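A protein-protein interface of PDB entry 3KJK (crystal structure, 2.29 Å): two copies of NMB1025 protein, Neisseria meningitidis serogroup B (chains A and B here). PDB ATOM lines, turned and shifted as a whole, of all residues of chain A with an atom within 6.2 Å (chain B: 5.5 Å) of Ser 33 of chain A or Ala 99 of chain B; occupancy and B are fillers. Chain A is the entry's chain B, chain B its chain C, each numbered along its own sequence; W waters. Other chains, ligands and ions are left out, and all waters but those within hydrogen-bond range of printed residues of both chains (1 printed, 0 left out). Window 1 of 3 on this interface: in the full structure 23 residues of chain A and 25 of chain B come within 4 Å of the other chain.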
ATOM      1  N   TYR A  20     -19.366   1.934 -17.674  1.00  0.00           N
ATOM      2  CA  TYR A  20     -18.624   2.686 -16.664  1.00  0.00           C
ATOM      3  C   TYR A  20     -17.126   2.586 -16.939  1.00  0.00           C
ATOM      4  O   TYR A  20     -16.692   1.758 -17.726  1.00  0.00           O
ATOM      5  CB  TYR A  20     -18.914   2.142 -15.257  1.00  0.00           C
ATOM      6  CG  TYR A  20     -18.442   0.719 -15.040  1.00  0.00           C
ATOM      7  CD1 TYR A  20     -17.128   0.450 -14.649  1.00  0.00           C
ATOM      8  CD2 TYR A  20     -19.306  -0.359 -15.230  1.00  0.00           C
ATOM      9  CE1 TYR A  20     -16.687  -0.848 -14.460  1.00  0.00           C
ATOM     10  CE2 TYR A  20     -18.873  -1.668 -15.043  1.00  0.00           C
ATOM     11  CZ  TYR A  20     -17.563  -1.904 -14.658  1.00  0.00           C
ATOM     12  OH  TYR A  20     -17.126  -3.192 -14.467  1.00  0.00           O
ATOM     13  N   SER A  21     -16.346   3.438 -16.289  1.00  0.00           N
ATOM     14  CA  SER A  21     -14.910   3.238 -16.234  1.00  0.00           C
ATOM     15  C   SER A  21     -14.529   2.895 -14.803  1.00  0.00           C
ATOM     16  O   SER A  21     -15.139   3.391 -13.858  1.00  0.00           O
ATOM     17  CB  SER A  21     -14.150   4.474 -16.718  1.00  0.00           C
ATOM     18  OG  SER A  21     -14.541   4.818 -18.033  1.00  0.00           O
ATOM     19  N   GLU A  22     -13.512   2.053 -14.657  1.00  0.00           N
ATOM     20  CA  GLU A  22     -13.088   1.583 -13.348  1.00  0.00           C
ATOM     21  C   GLU A  22     -12.456   2.716 -12.554  1.00  0.00           C
ATOM     22  O   GLU A  22     -12.533   2.741 -11.325  1.00  0.00           O
ATOM     23  CB  GLU A  22     -12.122   0.406 -13.484  1.00  0.00           C
ATOM     24  CG  GLU A  22     -12.741  -0.872 -14.057  1.00  0.00           C
ATOM     25  CD  GLU A  22     -13.687  -1.592 -13.086  1.00  0.00           C
ATOM     26  OE1 GLU A  22     -13.954  -1.070 -11.980  1.00  0.00           O
ATOM     27  OE2 GLU A  22     -14.172  -2.691 -13.445  1.00  0.00           O
ATOM     28  N   ALA A  23     -11.855   3.663 -13.270  1.00  0.00           N
ATOM     29  CA  ALA A  23     -11.272   4.848 -12.660  1.00  0.00           C
ATOM     30  C   ALA A  23     -11.299   6.002 -13.644  1.00  0.00           C
ATOM     31  O   ALA A  23     -11.090   5.812 -14.847  1.00  0.00           O
ATOM     32  CB  ALA A  23      -9.835   4.573 -12.215  1.00  0.00           C
ATOM     33  N   VAL A  24     -11.563   7.194 -13.113  1.00  0.00           N
ATOM     34  CA  VAL A  24     -11.519   8.434 -13.875  1.00  0.00           C
ATOM     35  C   VAL A  24     -10.658   9.416 -13.098  1.00  0.00           C
ATOM     36  O   VAL A  24     -10.824   9.568 -11.885  1.00  0.00           O
ATOM     37  CB  VAL A  24     -12.929   9.042 -14.083  1.00  0.00           C
ATOM     38  CG1 VAL A  24     -12.841  10.287 -14.920  1.00  0.00           C
ATOM     39  CG2 VAL A  24     -13.867   8.047 -14.743  1.00  0.00           C
ATOM     40  N   PHE A  31     -11.192   9.093  -9.194  1.00  0.00           N
ATOM     41  CA  PHE A  31     -12.464   8.545  -8.751  1.00  0.00           C
ATOM     42  C   PHE A  31     -12.570   7.100  -9.220  1.00  0.00           C
ATOM     43  O   PHE A  31     -12.571   6.830 -10.423  1.00  0.00           O
ATOM     44  CB  PHE A  31     -13.623   9.356  -9.339  1.00  0.00           C
ATOM     45  CG  PHE A  31     -13.738  10.748  -8.794  1.00  0.00           C
ATOM     46  CD1 PHE A  31     -14.652  11.036  -7.789  1.00  0.00           C
ATOM     47  CD2 PHE A  31     -12.948  11.777  -9.301  1.00  0.00           C
ATOM     48  CE1 PHE A  31     -14.767  12.322  -7.293  1.00  0.00           C
ATOM     49  CE2 PHE A  31     -13.056  13.067  -8.811  1.00  0.00           C
ATOM     50  CZ  PHE A  31     -13.967  13.342  -7.807  1.00  0.00           C
ATOM     51  N   LEU A  32     -12.648   6.169  -8.278  1.00  0.00           N
ATOM     52  CA  LEU A  32     -12.829   4.768  -8.636  1.00  0.00           C
ATOM     53  C   LEU A  32     -14.306   4.435  -8.671  1.00  0.00           C
ATOM     54  O   LEU A  32     -15.105   5.012  -7.922  1.00  0.00           O
ATOM     55  CB  LEU A  32     -12.127   3.841  -7.640  1.00  0.00           C
ATOM     56  CG  LEU A  32     -10.622   4.002  -7.359  1.00  0.00           C
ATOM     57  CD1 LEU A  32     -10.123   2.775  -6.608  1.00  0.00           C
ATOM     58  CD2 LEU A  32      -9.824   4.197  -8.633  1.00  0.00           C
ATOM     59  N   SER A  33     -14.672   3.502  -9.542  1.00  0.00           N
ATOM     60  CA  SER A  33     -16.004   2.917  -9.486  1.00  0.00           C
ATOM     61  C   SER A  33     -16.167   2.192  -8.162  1.00  0.00           C
ATOM     62  O   SER A  33     -15.178   1.854  -7.514  1.00  0.00           O
ATOM     63  CB  SER A  33     -16.185   1.930 -10.637  1.00  0.00           C
ATOM     64  OG  SER A  33     -16.630   2.601 -11.799  1.00  0.00           O
ATOM     65  N   GLY A  34     -17.405   1.950  -7.747  1.00  0.00           N
ATOM     66  CA  GLY A  34     -17.631   1.047  -6.624  1.00  0.00           C
ATOM     67  C   GLY A  34     -16.943  -0.271  -6.944  1.00  0.00           C
ATOM     68  O   GLY A  34     -17.150  -0.838  -8.022  1.00  0.00           O
ATOM     69  N   MET A  35     -16.091  -0.735  -6.036  1.00  0.00           N
ATOM     70  CA  MET A  35     -15.414  -2.017  -6.217  1.00  0.00           C
ATOM     71  C   MET A  35     -16.216  -3.110  -5.525  1.00  0.00           C
ATOM     72  O   MET A  35     -16.573  -2.986  -4.348  1.00  0.00           O
ATOM     73  CB  MET A  35     -13.986  -1.974  -5.679  1.00  0.00           C
ATOM     74  CG  MET A  35     -13.063  -1.033  -6.450  1.00  0.00           C
ATOM     75  SD  MET A  35     -12.737  -1.626  -8.279  1.00  0.00           S
ATOM     76  CE  MET A  35     -12.256   0.100  -9.083  1.00  0.00           C
ATOM     77  N   GLU A 115     -19.119  -3.331  -0.655  1.00  0.00           N
ATOM     78  CA  GLU A 115     -18.679  -2.550  -1.815  1.00  0.00           C
ATOM     79  C   GLU A 115     -18.053  -1.263  -1.323  1.00  0.00           C
ATOM     80  O   GLU A 115     -18.622  -0.581  -0.480  1.00  0.00           O
ATOM     81  CB  GLU A 115     -19.861  -2.238  -2.745  1.00  0.00           C
ATOM     82  CG  GLU A 115     -19.526  -1.284  -3.893  1.00  0.00           C
ATOM     83  CD  GLU A 115     -20.610  -1.199  -4.964  1.00  0.00           C
ATOM     84  OE1 GLU A 115     -21.592  -1.977  -4.934  1.00  0.00           O
ATOM     85  OE2 GLU A 115     -20.469  -0.345  -5.853  1.00  0.00           O
ATOM     86  N   ILE A 116     -16.885  -0.930  -1.853  1.00  0.00           N
ATOM     87  CA  ILE A 116     -16.129   0.226  -1.385  1.00  0.00           C
ATOM     88  C   ILE A 116     -15.891   1.243  -2.503  1.00  0.00           C
ATOM     89  O   ILE A 116     -15.393   0.897  -3.576  1.00  0.00           O
ATOM     90  CB  ILE A 116     -14.792  -0.209  -0.740  1.00  0.00           C
ATOM     91  CG1 ILE A 116     -15.062  -1.230   0.379  1.00  0.00           C
ATOM     92  CG2 ILE A 116     -14.035   1.000  -0.207  1.00  0.00           C
ATOM     93  CD1 ILE A 116     -13.850  -1.623   1.196  1.00  0.00           C
ATOM     94  N   LYS A 117     -16.256   2.497  -2.240  1.00  0.00           N
ATOM     95  CA  LYS A 117     -16.112   3.570  -3.219  1.00  0.00           C
ATOM     96  C   LYS A 117     -15.047   4.586  -2.832  1.00  0.00           C
ATOM     97  O   LYS A 117     -15.222   5.335  -1.875  1.00  0.00           O
ATOM     98  CB  LYS A 117     -17.440   4.275  -3.455  1.00  0.00           C
ATOM     99  CG  LYS A 117     -17.515   4.906  -4.814  1.00  0.00           C
ATOM    100  CD  LYS A 117     -18.524   6.011  -4.832  1.00  0.00           C
ATOM    101  CE  LYS A 117     -18.211   6.973  -5.943  1.00  0.00           C
ATOM    102  NZ  LYS A 117     -18.548   8.357  -5.530  1.00  0.00           N
ATOM    103  N   ILE A 118     -13.966   4.615  -3.605  1.00  0.00           N
ATOM    104  CA  ILE A 118     -12.768   5.393  -3.279  1.00  0.00           C
ATOM    105  C   ILE A 118     -12.640   6.687  -4.083  1.00  0.00           C
ATOM    106  O   ILE A 118     -12.971   6.727  -5.270  1.00  0.00           O
ATOM    107  CB  ILE A 118     -11.478   4.553  -3.502  1.00  0.00           C
ATOM    108  CG1 ILE A 118     -11.385   3.403  -2.490  1.00  0.00           C
ATOM    109  CG2 ILE A 118     -10.216   5.423  -3.441  1.00  0.00           C
ATOM    110  CD1 ILE A 118     -10.887   3.793  -1.082  1.00  0.00           C
ATOM    111  N   VAL B  68     -18.609  13.852 -17.205  1.00  0.00           N
ATOM    112  CA  VAL B  68     -18.985  13.349 -15.892  1.00  0.00           C
ATOM    113  C   VAL B  68     -17.867  12.464 -15.359  1.00  0.00           C
ATOM    114  O   VAL B  68     -17.322  11.633 -16.091  1.00  0.00           O
ATOM    115  CB  VAL B  68     -20.296  12.571 -15.950  1.00  0.00           C
ATOM    116  CG1 VAL B  68     -20.557  11.844 -14.629  1.00  0.00           C
ATOM    117  CG2 VAL B  68     -21.436  13.514 -16.273  1.00  0.00           C
ATOM    118  N   LEU B  69     -17.529  12.659 -14.086  1.00  0.00           N
ATOM    119  CA  LEU B  69     -16.461  11.907 -13.432  1.00  0.00           C
ATOM    120  C   LEU B  69     -17.002  10.710 -12.680  1.00  0.00           C
ATOM    121  O   LEU B  69     -16.391   9.640 -12.683  1.00  0.00           O
ATOM    122  CB  LEU B  69     -15.712  12.796 -12.438  1.00  0.00           C
ATOM    123  CG  LEU B  69     -14.987  14.038 -12.949  1.00  0.00           C
ATOM    124  CD1 LEU B  69     -14.379  14.759 -11.777  1.00  0.00           C
ATOM    125  CD2 LEU B  69     -13.928  13.659 -13.953  1.00  0.00           C
ATOM    126  N   ASP B  70     -18.158  10.900 -12.048  1.00  0.00           N
ATOM    127  CA  ASP B  70     -18.618  10.004 -11.005  1.00  0.00           C
ATOM    128  C   ASP B  70     -20.129  10.005 -10.909  1.00  0.00           C
ATOM    129  O   ASP B  70     -20.754  11.063 -10.981  1.00  0.00           O
ATOM    130  CB  ASP B  70     -18.028  10.458  -9.671  1.00  0.00           C
ATOM    131  CG  ASP B  70     -18.247   9.464  -8.575  1.00  0.00           C
ATOM    132  OD1 ASP B  70     -17.974   8.265  -8.800  1.00  0.00           O
ATOM    133  OD2 ASP B  70     -18.683   9.887  -7.483  1.00  0.00           O
ATOM    134  N   ALA B  71     -20.710   8.816 -10.748  1.00  0.00           N
ATOM    135  CA  ALA B  71     -22.152   8.679 -10.580  1.00  0.00           C
ATOM    136  C   ALA B  71     -22.481   7.614  -9.550  1.00  0.00           C
ATOM    137  O   ALA B  71     -22.079   6.462  -9.701  1.00  0.00           O
ATOM    138  CB  ALA B  71     -22.809   8.344 -11.892  1.00  0.00           C
ATOM    139  N   THR B  97     -17.368   6.936 -20.288  1.00  0.00           N
ATOM    140  CA  THR B  97     -18.273   6.489 -19.251  1.00  0.00           C
ATOM    141  C   THR B  97     -17.633   6.793 -17.900  1.00  0.00           C
ATOM    142  O   THR B  97     -16.415   6.639 -17.747  1.00  0.00           O
ATOM    143  CB  THR B  97     -18.569   4.990 -19.381  1.00  0.00           C
ATOM    144  OG1 THR B  97     -17.348   4.251 -19.299  1.00  0.00           O
ATOM    145  CG2 THR B  97     -19.229   4.690 -20.714  1.00  0.00           C
ATOM    146  N   PRO B  98     -18.443   7.240 -16.919  1.00  0.00           N
ATOM    147  CA  PRO B  98     -17.891   7.719 -15.653  1.00  0.00           C
ATOM    148  C   PRO B  98     -17.613   6.598 -14.660  1.00  0.00           C
ATOM    149  O   PRO B  98     -18.045   5.464 -14.878  1.00  0.00           O
ATOM    150  CB  PRO B  98     -19.013   8.609 -15.116  1.00  0.00           C
ATOM    151  CG  PRO B  98     -20.255   7.956 -15.611  1.00  0.00           C
ATOM    152  CD  PRO B  98     -19.913   7.374 -16.960  1.00  0.00           C
ATOM    153  N   ALA B  99     -16.886   6.910 -13.587  1.00  0.00           N
ATOM    154  CA  ALA B  99     -16.843   6.020 -12.437  1.00  0.00           C
ATOM    155  C   ALA B  99     -18.282   5.871 -11.962  1.00  0.00           C
ATOM    156  O   ALA B  99     -19.053   6.834 -12.015  1.00  0.00           O
ATOM    157  CB  ALA B  99     -15.983   6.602 -11.347  1.00  0.00           C
ATOM    158  N   ARG B 100     -18.652   4.672 -11.517  1.00  0.00           N
ATOM    159  CA  ARG B 100     -20.043   4.405 -11.142  1.00  0.00           C
ATOM    160  C   ARG B 100     -20.159   3.471  -9.942  1.00  0.00           C
ATOM    161  O   ARG B 100     -19.334   2.580  -9.751  1.00  0.00           O
ATOM    162  CB  ARG B 100     -20.834   3.833 -12.331  1.00  0.00           C
ATOM    163  CG  ARG B 100     -22.359   4.021 -12.213  1.00  0.00           C
ATOM    164  CD  ARG B 100     -23.148   3.315 -13.323  1.00  0.00           C
ATOM    165  NE  ARG B 100     -23.506   1.933 -12.982  1.00  0.00           N
ATOM    166  CZ  ARG B 100     -24.491   1.239 -13.553  1.00  0.00           C
ATOM    167  NH1 ARG B 100     -25.256   1.785 -14.497  1.00  0.00           N
ATOM    168  NH2 ARG B 100     -24.722  -0.012 -13.175  1.00  0.00           N
ATOM    169  N   ALA B 101     -21.190   3.706  -9.134  1.00  0.00           N
ATOM    170  CA  ALA B 101     -21.603   2.791  -8.081  1.00  0.00           C
ATOM    171  C   ALA B 101     -23.114   2.770  -8.074  1.00  0.00           C
ATOM    172  O   ALA B 101     -23.750   3.806  -8.294  1.00  0.00           O
ATOM    173  CB  ALA B 101     -21.085   3.250  -6.737  1.00  0.00           C
HETATM  174  O   HOH W   1     -19.296  -0.814  -9.713  1.00  0.00           O
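N of Ala 101 of chain B sits at hydrogen-bond distance from O of Ala 71 of chain B, at 3.0 Å. The backbone carbonyl oxygen (O) of Leu 69 of chain B lies within hydrogen-bond range of the backbone NH (N) of Ala 99 of chain B. N of Leu 32 of chain A is in hydrogen-bond range of O of Ile 118 of chain A (3.1 Å). The backbone carbonyl oxygen (O) of Val 24 of chain A is in hydrogen-bond range of the backbone NH (N) of Phe 31 of chain A (2.8 Å). The backbone carbonyl oxygen (O) of Ala 99 of chain B is in hydrogen-bond range of the backbone NH (N) of Ala 71 of chain B (2.9 Å). The backbone carbonyl oxygen (O) of Ser 21 of chain A lies within hydrogen-bond range of the side-chain hydroxyl (OG) of Ser 33 of chain A (2.7 Å).
Ala 23 of chain A touches none of the printed residues of chain B. Of chain B, only Ala 99 (3.5 Å) and Arg 100 (2.9 Å) come within 4 Å of Ser 33 of chain A. Of the printed residues of chain B, Glu 115 of chain A touches Ala 101. Val 68 of chain B touches none of the printed residues of chain A. Ala 99 of chain B touches just these residues of chain A: Ser 21, Val 24, Phe 31, Leu 32 and Ser 33. Of the printed residues of chain A, Arg 100 of chain B touches Tyr 20, Ser 33 and Gly 34. Printed residues of chain A within 4 Å of Ala 101 of chain B: Glu 115 (3.8 Å). The nearest residue of chain B that does not touch Ser 33 of chain A is Pro 98 of chain B (4.4 Å). The nearest residue of chain A that does not touch Ala 99 of chain B is Tyr 20 of chain A (5.0 Å). The nearest printed residue of chain B that does not touch Tyr 20 of chain A is Ala 99 of chain B (5.0 Å).
No position is printed for both chains.
The side-chain hydroxyl (OG) of Ser 33 of chain A sits at hydrogen-bond distance from the backbone NH (N) of Arg 100 of chain B, at 2.9 Å. O of Thr 97 of chain B is in hydrogen-bond range of OG of Ser 21 of chain A (2.6 Å). N of Ser 21 of chain A sits at hydrogen-bond distance from O of Pro 98 of chain B, at 3.0 Å. The side-chain carboxylate (OD2) of Asp 70 of chain B is in salt-bridge range of the side-chain amino group (NZ) of Lys 117 of chain A (2.5 Å). The backbone carbonyl oxygen (O) of Tyr 20 of chain A lies close to the side-chain hydroxyl (OG1) of Thr 97 of chain B, at 3.0 Å. N of Gly 34 of chain A is in hydrogen-bond range of O of Arg 100 of chain B (2.9 Å).
Water W1 bridges the backbone carbonyl oxygen (O) of Gly 34 of chain A (2.7 Å) and the backbone carbonyl oxygen (O) of Arg 100 of chain B (3.4 Å).
Printed residues of chain B that touch a printed residue of chain A: Leu 69, Asp 70, Thr 97, Pro 98, Ala 99, Arg 100 and Ala 101. Among the printed residues, Asp or Glu carboxylates within 4 Å of a Lys or Arg side-chain nitrogen of the other chain: Lys 117 of chain A with Asp 70 of chain B (2.5 Å).
CA of Tyr 20 of chain A touches O of Pro 98 of chain B, at 3.4 Å. Arg 100 of chain B touches Tyr 20 of chain A. Ser 21 of chain A touches Ala 99 of chain B. CG2 of Val 24 of chain A touches O of Leu 69 of chain B, at 3.6 Å. Val 24 of chain A touches Ala 99 of chain B (CG2 to N, 3.4 Å). Leu 69 of chain B touches Phe 31 of chain A. O of Phe 31 of chain A touches CB of Ala 99 of chain B (3.5 Å). C of Leu 32 of chain A touches CB of Ala 99 of chain B, 3.8 Å away. Ser 33 of chain A touches Ala 99 of chain B (OG to CA, 3.5 Å). Ala 101 of chain B touches Glu 115 of chain A (CB to OE2, 3.8 Å).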
